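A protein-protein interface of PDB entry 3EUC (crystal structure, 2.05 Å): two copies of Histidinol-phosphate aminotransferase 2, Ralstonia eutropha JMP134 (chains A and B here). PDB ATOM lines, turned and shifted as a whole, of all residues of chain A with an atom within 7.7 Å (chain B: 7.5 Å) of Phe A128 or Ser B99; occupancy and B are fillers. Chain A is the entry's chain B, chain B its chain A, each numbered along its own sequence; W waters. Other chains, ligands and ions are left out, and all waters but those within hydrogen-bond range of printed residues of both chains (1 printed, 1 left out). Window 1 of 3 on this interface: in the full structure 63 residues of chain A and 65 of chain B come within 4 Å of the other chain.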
ATOM      1  N   SER A  99      -7.054  -1.464  24.084  1.00  0.00           N
ATOM      2  CA  SER A  99      -6.776  -2.199  22.829  1.00  0.00           C
ATOM      3  C   SER A  99      -7.638  -1.724  21.679  1.00  0.00           C
ATOM      4  O   SER A  99      -7.128  -1.525  20.570  1.00  0.00           O
ATOM      5  CB  SER A  99      -6.965  -3.697  23.021  1.00  0.00           C
ATOM      6  OG  SER A  99      -6.165  -4.115  24.125  1.00  0.00           O
ATOM      7  N   ALA A 102      -6.449   1.718  20.365  1.00  0.00           N
ATOM      8  CA  ALA A 102      -5.236   1.540  19.574  1.00  0.00           C
ATOM      9  C   ALA A 102      -5.571   1.015  18.180  1.00  0.00           C
ATOM     10  O   ALA A 102      -5.047   1.521  17.204  1.00  0.00           O
ATOM     11  CB  ALA A 102      -4.220   0.623  20.285  1.00  0.00           C
ATOM     12  N   LEU A 103      -6.477   0.050  18.089  1.00  0.00           N
ATOM     13  CA  LEU A 103      -6.867  -0.530  16.788  1.00  0.00           C
ATOM     14  C   LEU A 103      -7.620   0.481  15.903  1.00  0.00           C
ATOM     15  O   LEU A 103      -7.278   0.646  14.725  1.00  0.00           O
ATOM     16  CB  LEU A 103      -7.709  -1.808  16.998  1.00  0.00           C
ATOM     17  CG  LEU A 103      -8.093  -2.627  15.752  1.00  0.00           C
ATOM     18  CD1 LEU A 103      -6.862  -3.002  14.914  1.00  0.00           C
ATOM     19  CD2 LEU A 103      -8.882  -3.872  16.165  1.00  0.00           C
ATOM     20  N   MET A 121      -0.026  -1.129  29.820  1.00  0.00           N
ATOM     21  CA  MET A 121      -0.877  -1.286  28.635  1.00  0.00           C
ATOM     22  C   MET A 121      -0.930  -0.131  27.669  1.00  0.00           C
ATOM     23  O   MET A 121      -1.326  -0.343  26.518  1.00  0.00           O
ATOM     24  CB  MET A 121      -2.292  -1.709  29.029  1.00  0.00           C
ATOM     25  CG  MET A 121      -2.345  -3.149  29.545  1.00  0.00           C
ATOM     26  SD  MET A 121      -2.012  -4.397  28.051  1.00  0.00           S
ATOM     27  CE  MET A 121      -3.461  -3.906  26.966  1.00  0.00           C
ATOM     28  N   TYR A 122      -0.524   1.074  28.062  1.00  0.00           N
ATOM     29  CA  TYR A 122      -0.527   2.192  27.066  1.00  0.00           C
ATOM     30  C   TYR A 122       0.525   1.869  25.985  1.00  0.00           C
ATOM     31  O   TYR A 122       0.205   1.843  24.790  1.00  0.00           O
ATOM     32  CB  TYR A 122      -0.299   3.576  27.698  1.00  0.00           C
ATOM     33  CG  TYR A 122      -1.145   3.888  28.930  1.00  0.00           C
ATOM     34  CD1 TYR A 122      -2.507   3.540  28.992  1.00  0.00           C
ATOM     35  CD2 TYR A 122      -0.605   4.614  29.999  1.00  0.00           C
ATOM     36  CE1 TYR A 122      -3.292   3.844  30.139  1.00  0.00           C
ATOM     37  CE2 TYR A 122      -1.378   4.939  31.138  1.00  0.00           C
ATOM     38  CZ  TYR A 122      -2.713   4.544  31.198  1.00  0.00           C
ATOM     39  OH  TYR A 122      -3.458   4.849  32.288  1.00  0.00           O
ATOM     40  N   ALA A 123       1.756   1.588  26.416  1.00  0.00           N
ATOM     41  CA  ALA A 123       2.863   1.181  25.527  1.00  0.00           C
ATOM     42  C   ALA A 123       2.612  -0.177  24.868  1.00  0.00           C
ATOM     43  O   ALA A 123       2.864  -0.345  23.667  1.00  0.00           O
ATOM     44  CB  ALA A 123       4.183   1.137  26.311  1.00  0.00           C
ATOM     45  N   MET A 124       2.099  -1.129  25.651  1.00  0.00           N
ATOM     46  CA  MET A 124       1.810  -2.491  25.168  1.00  0.00           C
ATOM     47  C   MET A 124       0.726  -2.517  24.084  1.00  0.00           C
ATOM     48  O   MET A 124       0.897  -3.182  23.043  1.00  0.00           O
ATOM     49  CB  MET A 124       1.388  -3.382  26.316  1.00  0.00           C
ATOM     50  CG  MET A 124       1.461  -4.845  26.045  1.00  0.00           C
ATOM     51  SD  MET A 124       3.100  -5.585  26.659  1.00  0.00           S
ATOM     52  CE  MET A 124       4.516  -4.541  25.626  1.00  0.00           C
ATOM     53  N   SER A 125      -0.369  -1.794  24.311  1.00  0.00           N
ATOM     54  CA  SER A 125      -1.446  -1.701  23.323  1.00  0.00           C
ATOM     55  C   SER A 125      -0.893  -1.136  22.004  1.00  0.00           C
ATOM     56  O   SER A 125      -1.248  -1.618  20.935  1.00  0.00           O
ATOM     57  CB  SER A 125      -2.620  -0.825  23.800  1.00  0.00           C
ATOM     58  OG  SER A 125      -2.260   0.555  23.891  1.00  0.00           O
ATOM     59  N   ALA A 126      -0.026  -0.122  22.107  1.00  0.00           N
ATOM     60  CA  ALA A 126       0.619   0.490  20.935  1.00  0.00           C
ATOM     61  C   ALA A 126       1.503  -0.538  20.199  1.00  0.00           C
ATOM     62  O   ALA A 126       1.436  -0.642  18.959  1.00  0.00           O
ATOM     63  CB  ALA A 126       1.432   1.728  21.343  1.00  0.00           C
ATOM     64  N   GLN A 127       2.274  -1.320  20.962  1.00  0.00           N
ATOM     65  CA  GLN A 127       3.182  -2.331  20.397  1.00  0.00           C
ATOM     66  C   GLN A 127       2.421  -3.439  19.680  1.00  0.00           C
ATOM     67  O   GLN A 127       2.819  -3.842  18.580  1.00  0.00           O
ATOM     68  CB  GLN A 127       4.114  -2.956  21.464  1.00  0.00           C
ATOM     69  CG  GLN A 127       5.324  -3.706  20.816  1.00  0.00           C
ATOM     70  CD  GLN A 127       6.302  -4.327  21.824  1.00  0.00           C
ATOM     71  OE1 GLN A 127       5.945  -4.604  22.969  1.00  0.00           O
ATOM     72  NE2 GLN A 127       7.543  -4.568  21.375  1.00  0.00           N
ATOM     73  N   PHE A 128       1.344  -3.917  20.314  1.00  0.00           N
ATOM     74  CA  PHE A 128       0.474  -4.942  19.730  1.00  0.00           C
ATOM     75  C   PHE A 128      -0.264  -4.466  18.477  1.00  0.00           C
ATOM     76  O   PHE A 128      -0.589  -5.302  17.629  1.00  0.00           O
ATOM     77  CB  PHE A 128      -0.522  -5.533  20.741  1.00  0.00           C
ATOM     78  CG  PHE A 128       0.048  -6.647  21.604  1.00  0.00           C
ATOM     79  CD1 PHE A 128       0.177  -7.935  21.091  1.00  0.00           C
ATOM     80  CD2 PHE A 128       0.389  -6.432  22.932  1.00  0.00           C
ATOM     81  CE1 PHE A 128       0.669  -9.005  21.873  1.00  0.00           C
ATOM     82  CE2 PHE A 128       0.887  -7.489  23.737  1.00  0.00           C
ATOM     83  CZ  PHE A 128       1.028  -8.780  23.195  1.00  0.00           C
ATOM     84  N   ALA A 129      -0.527  -3.152  18.374  1.00  0.00           N
ATOM     85  CA  ALA A 129      -1.162  -2.537  17.188  1.00  0.00           C
ATOM     86  C   ALA A 129      -0.135  -2.026  16.148  1.00  0.00           C
ATOM     87  O   ALA A 129      -0.524  -1.492  15.115  1.00  0.00           O
ATOM     88  CB  ALA A 129      -2.089  -1.405  17.616  1.00  0.00           C
ATOM     89  N   GLY A 130       1.162  -2.199  16.417  1.00  0.00           N
ATOM     90  CA  GLY A 130       2.232  -1.717  15.550  1.00  0.00           C
ATOM     91  C   GLY A 130       2.392  -0.199  15.503  1.00  0.00           C
ATOM     92  O   GLY A 130       2.797   0.347  14.471  1.00  0.00           O
ATOM     93  N   LEU A 131       2.065   0.473  16.604  1.00  0.00           N
ATOM     94  CA  LEU A 131       2.136   1.929  16.710  1.00  0.00           C
ATOM     95  C   LEU A 131       3.275   2.327  17.606  1.00  0.00           C
ATOM     96  O   LEU A 131       3.607   1.622  18.539  1.00  0.00           O
ATOM     97  CB  LEU A 131       0.837   2.495  17.281  1.00  0.00           C
ATOM     98  CG  LEU A 131      -0.465   2.162  16.540  1.00  0.00           C
ATOM     99  CD1 LEU A 131      -1.621   2.905  17.224  1.00  0.00           C
ATOM    100  CD2 LEU A 131      -0.379   2.495  15.061  1.00  0.00           C
ATOM    101  N   SER B  94      -9.080 -15.959  19.721  1.00  0.00           N
ATOM    102  CA  SER B  94      -8.101 -16.180  18.674  1.00  0.00           C
ATOM    103  C   SER B  94      -7.228 -14.932  18.420  1.00  0.00           C
ATOM    104  O   SER B  94      -6.051 -15.102  18.084  1.00  0.00           O
ATOM    105  CB  SER B  94      -8.760 -16.707  17.382  1.00  0.00           C
ATOM    106  OG  SER B  94      -9.586 -15.734  16.777  1.00  0.00           O
ATOM    107  N   ASP B  95      -7.785 -13.725  18.641  1.00  0.00           N
ATOM    108  CA  ASP B  95      -7.082 -12.454  18.350  1.00  0.00           C
ATOM    109  C   ASP B  95      -5.802 -12.258  19.152  1.00  0.00           C
ATOM    110  O   ASP B  95      -4.812 -11.754  18.602  1.00  0.00           O
ATOM    111  CB  ASP B  95      -7.997 -11.222  18.540  1.00  0.00           C
ATOM    112  CG  ASP B  95      -9.161 -11.162  17.535  1.00  0.00           C
ATOM    113  OD1 ASP B  95      -9.245 -12.005  16.613  1.00  0.00           O
ATOM    114  OD2 ASP B  95     -10.003 -10.249  17.687  1.00  0.00           O
ATOM    115  N   GLU B  96      -5.832 -12.642  20.425  1.00  0.00           N
ATOM    116  CA  GLU B  96      -4.667 -12.555  21.298  1.00  0.00           C
ATOM    117  C   GLU B  96      -3.519 -13.432  20.775  1.00  0.00           C
ATOM    118  O   GLU B  96      -2.372 -12.984  20.736  1.00  0.00           O
ATOM    119  CB  GLU B  96      -5.008 -13.009  22.726  1.00  0.00           C
ATOM    120  CG  GLU B  96      -3.898 -12.762  23.732  1.00  0.00           C
ATOM    121  CD  GLU B  96      -4.278 -13.192  25.142  1.00  0.00           C
ATOM    122  OE1 GLU B  96      -4.212 -14.390  25.445  1.00  0.00           O
ATOM    123  OE2 GLU B  96      -4.616 -12.333  25.967  1.00  0.00           O
ATOM    124  N   ILE B  97      -3.863 -14.664  20.380  1.00  0.00           N
ATOM    125  CA  ILE B  97      -2.905 -15.649  19.866  1.00  0.00           C
ATOM    126  C   ILE B  97      -2.304 -15.130  18.544  1.00  0.00           C
ATOM    127  O   ILE B  97      -1.094 -15.187  18.350  1.00  0.00           O
ATOM    128  CB  ILE B  97      -3.557 -17.050  19.658  1.00  0.00           C
ATOM    129  CG1 ILE B  97      -4.181 -17.624  20.949  1.00  0.00           C
ATOM    130  CG2 ILE B  97      -2.543 -18.042  19.073  1.00  0.00           C
ATOM    131  CD1 ILE B  97      -3.210 -17.930  22.042  1.00  0.00           C
ATOM    132  N   ILE B  98      -3.145 -14.630  17.649  1.00  0.00           N
ATOM    133  CA  ILE B  98      -2.659 -14.027  16.385  1.00  0.00           C
ATOM    134  C   ILE B  98      -1.696 -12.854  16.679  1.00  0.00           C
ATOM    135  O   ILE B  98      -0.627 -12.748  16.063  1.00  0.00           O
ATOM    136  CB  ILE B  98      -3.821 -13.545  15.481  1.00  0.00           C
ATOM    137  CG1 ILE B  98      -4.599 -14.728  14.924  1.00  0.00           C
ATOM    138  CG2 ILE B  98      -3.312 -12.705  14.296  1.00  0.00           C
ATOM    139  CD1 ILE B  98      -5.869 -14.308  14.182  1.00  0.00           C
ATOM    140  N   SER B  99      -2.065 -12.012  17.641  1.00  0.00           N
ATOM    141  CA  SER B  99      -1.237 -10.870  18.025  1.00  0.00           C
ATOM    142  C   SER B  99       0.074 -11.308  18.678  1.00  0.00           C
ATOM    143  O   SER B  99       1.114 -10.729  18.399  1.00  0.00           O
ATOM    144  CB  SER B  99      -2.005  -9.911  18.936  1.00  0.00           C
ATOM    145  OG  SER B  99      -3.183  -9.426  18.314  1.00  0.00           O
ATOM    146  N   MET B 100       0.015 -12.325  19.542  1.00  0.00           N
ATOM    147  CA  MET B 100       1.226 -12.886  20.169  1.00  0.00           C
ATOM    148  C   MET B 100       2.198 -13.442  19.130  1.00  0.00           C
ATOM    149  O   MET B 100       3.414 -13.231  19.260  1.00  0.00           O
ATOM    150  CB  MET B 100       0.888 -13.960  21.194  1.00  0.00           C
ATOM    151  CG  MET B 100       0.371 -13.389  22.452  1.00  0.00           C
ATOM    152  SD  MET B 100      -0.320 -14.724  23.602  1.00  0.00           S
ATOM    153  CE  MET B 100       1.309 -15.907  23.862  1.00  0.00           C
ATOM    154  N   LEU B 101       1.653 -14.160  18.135  1.00  0.00           N
ATOM    155  CA  LEU B 101       2.418 -14.716  17.013  1.00  0.00           C
ATOM    156  C   LEU B 101       3.110 -13.635  16.226  1.00  0.00           C
ATOM    157  O   LEU B 101       4.304 -13.728  15.976  1.00  0.00           O
ATOM    158  CB  LEU B 101       1.523 -15.527  16.045  1.00  0.00           C
ATOM    159  CG  LEU B 101       1.194 -16.976  16.365  1.00  0.00           C
ATOM    160  CD1 LEU B 101      -0.026 -17.481  15.568  1.00  0.00           C
ATOM    161  CD2 LEU B 101       2.445 -17.812  16.076  1.00  0.00           C
ATOM    162  N   ALA B 102       2.333 -12.648  15.779  1.00  0.00           N
ATOM    163  CA  ALA B 102       2.863 -11.519  15.028  1.00  0.00           C
ATOM    164  C   ALA B 102       3.955 -10.805  15.827  1.00  0.00           C
ATOM    165  O   ALA B 102       5.019 -10.549  15.298  1.00  0.00           O
ATOM    166  CB  ALA B 102       1.745 -10.543  14.636  1.00  0.00           C
ATOM    167  N   LEU B 103       3.699 -10.546  17.105  1.00  0.00           N
ATOM    168  CA  LEU B 103       4.650  -9.866  17.964  1.00  0.00           C
ATOM    169  C   LEU B 103       5.951 -10.670  18.129  1.00  0.00           C
ATOM    170  O   LEU B 103       7.029 -10.128  17.911  1.00  0.00           O
ATOM    171  CB  LEU B 103       4.023  -9.536  19.326  1.00  0.00           C
ATOM    172  CG  LEU B 103       4.754  -8.566  20.259  1.00  0.00           C
ATOM    173  CD1 LEU B 103       5.075  -7.258  19.554  1.00  0.00           C
ATOM    174  CD2 LEU B 103       3.873  -8.295  21.478  1.00  0.00           C
ATOM    175  N   ALA B 104       5.843 -11.966  18.398  1.00  0.00           N
ATOM    176  CA  ALA B 104       7.017 -12.851  18.518  1.00  0.00           C
ATOM    177  C   ALA B 104       7.902 -12.828  17.270  1.00  0.00           C
ATOM    178  O   ALA B 104       9.125 -12.966  17.375  1.00  0.00           O
ATOM    179  CB  ALA B 104       6.598 -14.304  18.852  1.00  0.00           C
ATOM    180  N   ALA B 105       7.274 -12.638  16.110  1.00  0.00           N
ATOM    181  CA  ALA B 105       7.932 -12.558  14.798  1.00  0.00           C
ATOM    182  C   ALA B 105       8.189 -11.124  14.281  1.00  0.00           C
ATOM    183  O   ALA B 105       8.560 -10.944  13.100  1.00  0.00           O
ATOM    184  CB  ALA B 105       7.047 -13.310  13.764  1.00  0.00           C
ATOM    185  N   ALA B 106       8.036 -10.110  15.139  1.00  0.00           N
ATOM    186  CA  ALA B 106       8.147  -8.700  14.723  1.00  0.00           C
ATOM    187  C   ALA B 106       9.614  -8.304  14.641  1.00  0.00           C
ATOM    188  O   ALA B 106      10.148  -7.601  15.502  1.00  0.00           O
ATOM    189  CB  ALA B 106       7.358  -7.777  15.668  1.00  0.00           C
ATOM    190  N   SER B 125      -2.292  -5.032   9.120  1.00  0.00           N
ATOM    191  CA  SER B 125      -0.966  -4.760   9.735  1.00  0.00           C
ATOM    192  C   SER B 125      -1.077  -4.480  11.269  1.00  0.00           C
ATOM    193  O   SER B 125      -0.266  -4.977  12.064  1.00  0.00           O
ATOM    194  CB  SER B 125      -0.270  -3.602   8.990  1.00  0.00           C
ATOM    195  OG  SER B 125       1.055  -3.416   9.441  1.00  0.00           O
ATOM    196  N   ALA B 126      -2.116  -3.722  11.645  1.00  0.00           N
ATOM    197  CA  ALA B 126      -2.475  -3.445  13.041  1.00  0.00           C
ATOM    198  C   ALA B 126      -2.833  -4.737  13.792  1.00  0.00           C
ATOM    199  O   ALA B 126      -2.418  -4.934  14.940  1.00  0.00           O
ATOM    200  CB  ALA B 126      -3.649  -2.442  13.114  1.00  0.00           C
ATOM    201  N   GLN B 127      -3.581  -5.624  13.135  1.00  0.00           N
ATOM    202  CA  GLN B 127      -3.944  -6.918  13.734  1.00  0.00           C
ATOM    203  C   GLN B 127      -2.788  -7.954  13.692  1.00  0.00           C
ATOM    204  O   GLN B 127      -2.916  -9.037  14.290  1.00  0.00           O
ATOM    205  CB  GLN B 127      -5.275  -7.425  13.156  1.00  0.00           C
ATOM    206  CG  GLN B 127      -6.425  -6.404  13.459  1.00  0.00           C
ATOM    207  CD  GLN B 127      -7.847  -6.938  13.309  1.00  0.00           C
ATOM    208  OE1 GLN B 127      -8.652  -6.371  12.558  1.00  0.00           O
ATOM    209  NE2 GLN B 127      -8.173  -8.011  14.044  1.00  0.00           N
ATOM    210  N   PHE B 128      -1.679  -7.602  13.007  1.00  0.00           N
ATOM    211  CA  PHE B 128      -0.450  -8.384  12.938  1.00  0.00           C
ATOM    212  C   PHE B 128       0.764  -7.596  13.476  1.00  0.00           C
ATOM    213  O   PHE B 128       1.804  -7.526  12.827  1.00  0.00           O
ATOM    214  CB  PHE B 128      -0.217  -8.867  11.496  1.00  0.00           C
ATOM    215  CG  PHE B 128      -1.266  -9.833  11.002  1.00  0.00           C
ATOM    216  CD1 PHE B 128      -1.444 -11.083  11.636  1.00  0.00           C
ATOM    217  CD2 PHE B 128      -2.048  -9.531   9.884  1.00  0.00           C
ATOM    218  CE1 PHE B 128      -2.423 -11.995  11.166  1.00  0.00           C
ATOM    219  CE2 PHE B 128      -3.016 -10.429   9.407  1.00  0.00           C
ATOM    220  CZ  PHE B 128      -3.206 -11.663  10.045  1.00  0.00           C
ATOM    221  N   ALA B 129       0.610  -6.991  14.659  1.00  0.00           N
ATOM    222  CA  ALA B 129       1.684  -6.270  15.389  1.00  0.00           C
ATOM    223  C   ALA B 129       2.590  -5.341  14.582  1.00  0.00           C
ATOM    224  O   ALA B 129       3.795  -5.266  14.846  1.00  0.00           O
ATOM    225  CB  ALA B 129       2.547  -7.289  16.184  1.00  0.00           C
ATOM    226  N   GLY B 130       2.016  -4.650  13.602  1.00  0.00           N
ATOM    227  CA  GLY B 130       2.783  -3.761  12.724  1.00  0.00           C
ATOM    228  C   GLY B 130       3.555  -4.413  11.581  1.00  0.00           C
ATOM    229  O   GLY B 130       4.165  -3.693  10.795  1.00  0.00           O
ATOM    230  N   LEU B 131       3.540  -5.750  11.466  1.00  0.00           N
ATOM    231  CA  LEU B 131       4.219  -6.443  10.359  1.00  0.00           C
ATOM    232  C   LEU B 131       3.518  -6.050   9.054  1.00  0.00           C
ATOM    233  O   LEU B 131       2.317  -5.811   9.056  1.00  0.00           O
ATOM    234  CB  LEU B 131       4.216  -7.972  10.519  1.00  0.00           C
ATOM    235  CG  LEU B 131       5.221  -8.633  11.477  1.00  0.00           C
ATOM    236  CD1 LEU B 131       5.092  -8.142  12.904  1.00  0.00           C
ATOM    237  CD2 LEU B 131       5.040 -10.125  11.446  1.00  0.00           C
ATOM    238  N   MET B 222      -4.334 -23.331  15.260  1.00  0.00           N
ATOM    239  CA  MET B 222      -5.088 -22.599  16.277  1.00  0.00           C
ATOM    240  C   MET B 222      -6.602 -22.800  16.133  1.00  0.00           C
ATOM    241  O   MET B 222      -7.145 -22.911  15.031  1.00  0.00           O
ATOM    242  CB  MET B 222      -4.702 -21.122  16.315  1.00  0.00           C
ATOM    243  CG  MET B 222      -5.032 -20.356  15.124  1.00  0.00           C
ATOM    244  SD  MET B 222      -4.531 -18.498  15.256  1.00  0.00           S
ATOM    245  CE  MET B 222      -5.565 -18.044  16.809  1.00  0.00           C
ATOM    246  N   LEU B 248       6.730 -18.292  21.645  1.00  0.00           N
ATOM    247  CA  LEU B 248       5.454 -17.556  21.592  1.00  0.00           C
ATOM    248  C   LEU B 248       4.902 -17.167  22.985  1.00  0.00           C
ATOM    249  O   LEU B 248       4.398 -16.068  23.195  1.00  0.00           O
ATOM    250  CB  LEU B 248       4.437 -18.374  20.775  1.00  0.00           C
ATOM    251  CG  LEU B 248       3.031 -17.828  20.529  1.00  0.00           C
ATOM    252  CD1 LEU B 248       3.075 -16.511  19.824  1.00  0.00           C
ATOM    253  CD2 LEU B 248       2.228 -18.845  19.729  1.00  0.00           C
ATOM    254  N   VAL B 251       5.872 -13.640  24.829  1.00  0.00           N
ATOM    255  CA  VAL B 251       5.287 -12.347  24.435  1.00  0.00           C
ATOM    256  C   VAL B 251       3.791 -12.198  24.812  1.00  0.00           C
ATOM    257  O   VAL B 251       3.102 -11.335  24.276  1.00  0.00           O
ATOM    258  CB  VAL B 251       5.522 -12.060  22.944  1.00  0.00           C
ATOM    259  CG1 VAL B 251       7.010 -12.166  22.627  1.00  0.00           C
ATOM    260  CG2 VAL B 251       4.708 -12.996  22.063  1.00  0.00           C
ATOM    261  N   ARG B 252       3.312 -13.018  25.747  1.00  0.00           N
ATOM    262  CA  ARG B 252       1.943 -12.932  26.271  1.00  0.00           C
ATOM    263  C   ARG B 252       1.709 -11.551  26.924  1.00  0.00           C
ATOM    264  O   ARG B 252       2.627 -11.031  27.546  1.00  0.00           O
ATOM    265  CB  ARG B 252       1.739 -14.036  27.325  1.00  0.00           C
ATOM    266  CG  ARG B 252       0.373 -14.073  28.031  1.00  0.00           C
ATOM    267  CD  ARG B 252       0.281 -15.258  29.003  1.00  0.00           C
ATOM    268  NE  ARG B 252       0.350 -16.499  28.246  1.00  0.00           N
ATOM    269  CZ  ARG B 252      -0.651 -17.012  27.522  1.00  0.00           C
ATOM    270  NH1 ARG B 252      -1.851 -16.416  27.462  1.00  0.00           N
ATOM    271  NH2 ARG B 252      -0.437 -18.136  26.838  1.00  0.00           N
ATOM    272  N   PRO B 253       0.506 -10.943  26.771  1.00  0.00           N
ATOM    273  CA  PRO B 253       0.260  -9.661  27.465  1.00  0.00           C
ATOM    274  C   PRO B 253       0.307  -9.775  28.995  1.00  0.00           C
ATOM    275  O   PRO B 253       0.234 -10.886  29.517  1.00  0.00           O
ATOM    276  CB  PRO B 253      -1.147  -9.269  27.003  1.00  0.00           C
ATOM    277  CG  PRO B 253      -1.370 -10.024  25.742  1.00  0.00           C
ATOM    278  CD  PRO B 253      -0.648 -11.318  25.927  1.00  0.00           C
ATOM    279  N   PRO B 254       0.373  -8.634  29.720  1.00  0.00           N
ATOM    280  CA  PRO B 254       0.487  -8.646  31.182  1.00  0.00           C
ATOM    281  C   PRO B 254      -0.861  -8.902  31.884  1.00  0.00           C
ATOM    282  O   PRO B 254      -1.315  -8.119  32.727  1.00  0.00           O
ATOM    283  CB  PRO B 254       1.092  -7.266  31.479  1.00  0.00           C
ATOM    284  CG  PRO B 254       0.491  -6.390  30.446  1.00  0.00           C
ATOM    285  CD  PRO B 254       0.320  -7.250  29.203  1.00  0.00           C
ATOM    286  N   TYR B 255      -1.454 -10.041  31.528  1.00  0.00           N
ATOM    287  CA  TYR B 255      -2.731 -10.544  32.036  1.00  0.00           C
ATOM    288  C   TYR B 255      -2.924 -11.971  31.507  1.00  0.00           C
ATOM    289  O   TYR B 255      -2.522 -12.298  30.374  1.00  0.00           O
ATOM    290  CB  TYR B 255      -3.935  -9.650  31.668  1.00  0.00           C
ATOM    291  CG  TYR B 255      -4.138  -9.316  30.200  1.00  0.00           C
ATOM    292  CD1 TYR B 255      -4.793 -10.195  29.338  1.00  0.00           C
ATOM    293  CD2 TYR B 255      -3.735  -8.073  29.681  1.00  0.00           C
ATOM    294  CE1 TYR B 255      -5.002  -9.865  27.976  1.00  0.00           C
ATOM    295  CE2 TYR B 255      -3.951  -7.736  28.331  1.00  0.00           C
ATOM    296  CZ  TYR B 255      -4.579  -8.636  27.491  1.00  0.00           C
ATOM    297  OH  TYR B 255      -4.775  -8.303  26.169  1.00  0.00           O
HETATM  298  O   HOH W   1      -6.622  -6.011  25.888  1.00  0.00           O
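Leu A103 touches Gln B127, and with the chains exchanged Gln A127 touches Leu B103.
Phe A128 touches Leu B103, but with the chains exchanged Leu A103 does not touch Phe B128 (7.2 Å).
Phe A128 touches Ala B126, but with the chains exchanged Ala A126 does not touch Phe B128 (8.9 Å).
Gly A130 touches Ala B129, but with the chains exchanged Ala A129 does not touch Gly B130 (4.2 Å).
The backbone carbonyl oxygen (O) of Phe A128 sits close to the backbone carbonyl oxygen (O) of Ala B126 (3.3 Å).
O of Asp B95 sits at hydrogen-bond distance from OG of Ser B99 (2.9 Å).
N of Gly B130 is in hydrogen-bond range of O of Ser B125 (2.8 Å).
O of Met A121 is in hydrogen-bond range of OG of Ser A125, 2.9 Å away.
Of the 14 printed residues of chain A, 6 touch a printed residue of chain B.
Of the 27 printed residues of chain B, 10 touch a printed residue of chain A.
Printed residues of chain B that touch a printed residue of chain A: Ser B99, Leu B103, Ala B126, Gln B127, Ala B129, Gly B130, Val B251, Pro B253, Pro B254 and Tyr B255.
Hydrophobic or aromatic side chains of chain B that line the printed part of chain A: Leu B103, Ala B126, Ala B129, Pro B253, Pro B254 and Tyr B255.
Among the printed residues, 14 pairs touch across the chains.
Water W1 bridges OG of Ser A99 (2.6 Å) and OH of Tyr B255 (3.0 Å).
Ser B99 touches just one residue of chain A: Phe A128.
Of the printed residues of chain B, Ala A129 touches Ala B126.
Printed residues of chain A within 4 Å of Tyr B255: Met A121 (3.9 Å).
Of the printed residues of chain A, Ala B129 touches Phe A128 and Gly A130.
Of the printed residues of chain A, Ala B126 touches Leu A103 (3.7 Å), Phe A128 (3.3 Å) and Ala A129 (3.5 Å).
Ala B102 touches none of the printed residues of chain A.
Among the printed residues, pairs that only touch across the chains: Leu A103 with Ala B126 (3.7 Å), Leu A103 with Gln B127 (3.7 Å), Met A121 with Pro B254 (3.9 Å), Met A121 with Tyr B255 (3.9 Å), Gln A127 with Leu B103 (3.8 Å), Phe A128 with Ser B99 (3.6 Å), Phe A128 with Leu B103 (3.3 Å), Phe A128 with Ala B129 (3.3 Å), Phe A128 with Val B251 (3.5 Å), Phe A128 with Pro B253 (3.7 Å), Ala A129 with Ala B126 (3.5 Å), Gly A130 with Ala B129 (3.8 Å) and Gly A130 with Gly B130 (3.5 Å).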
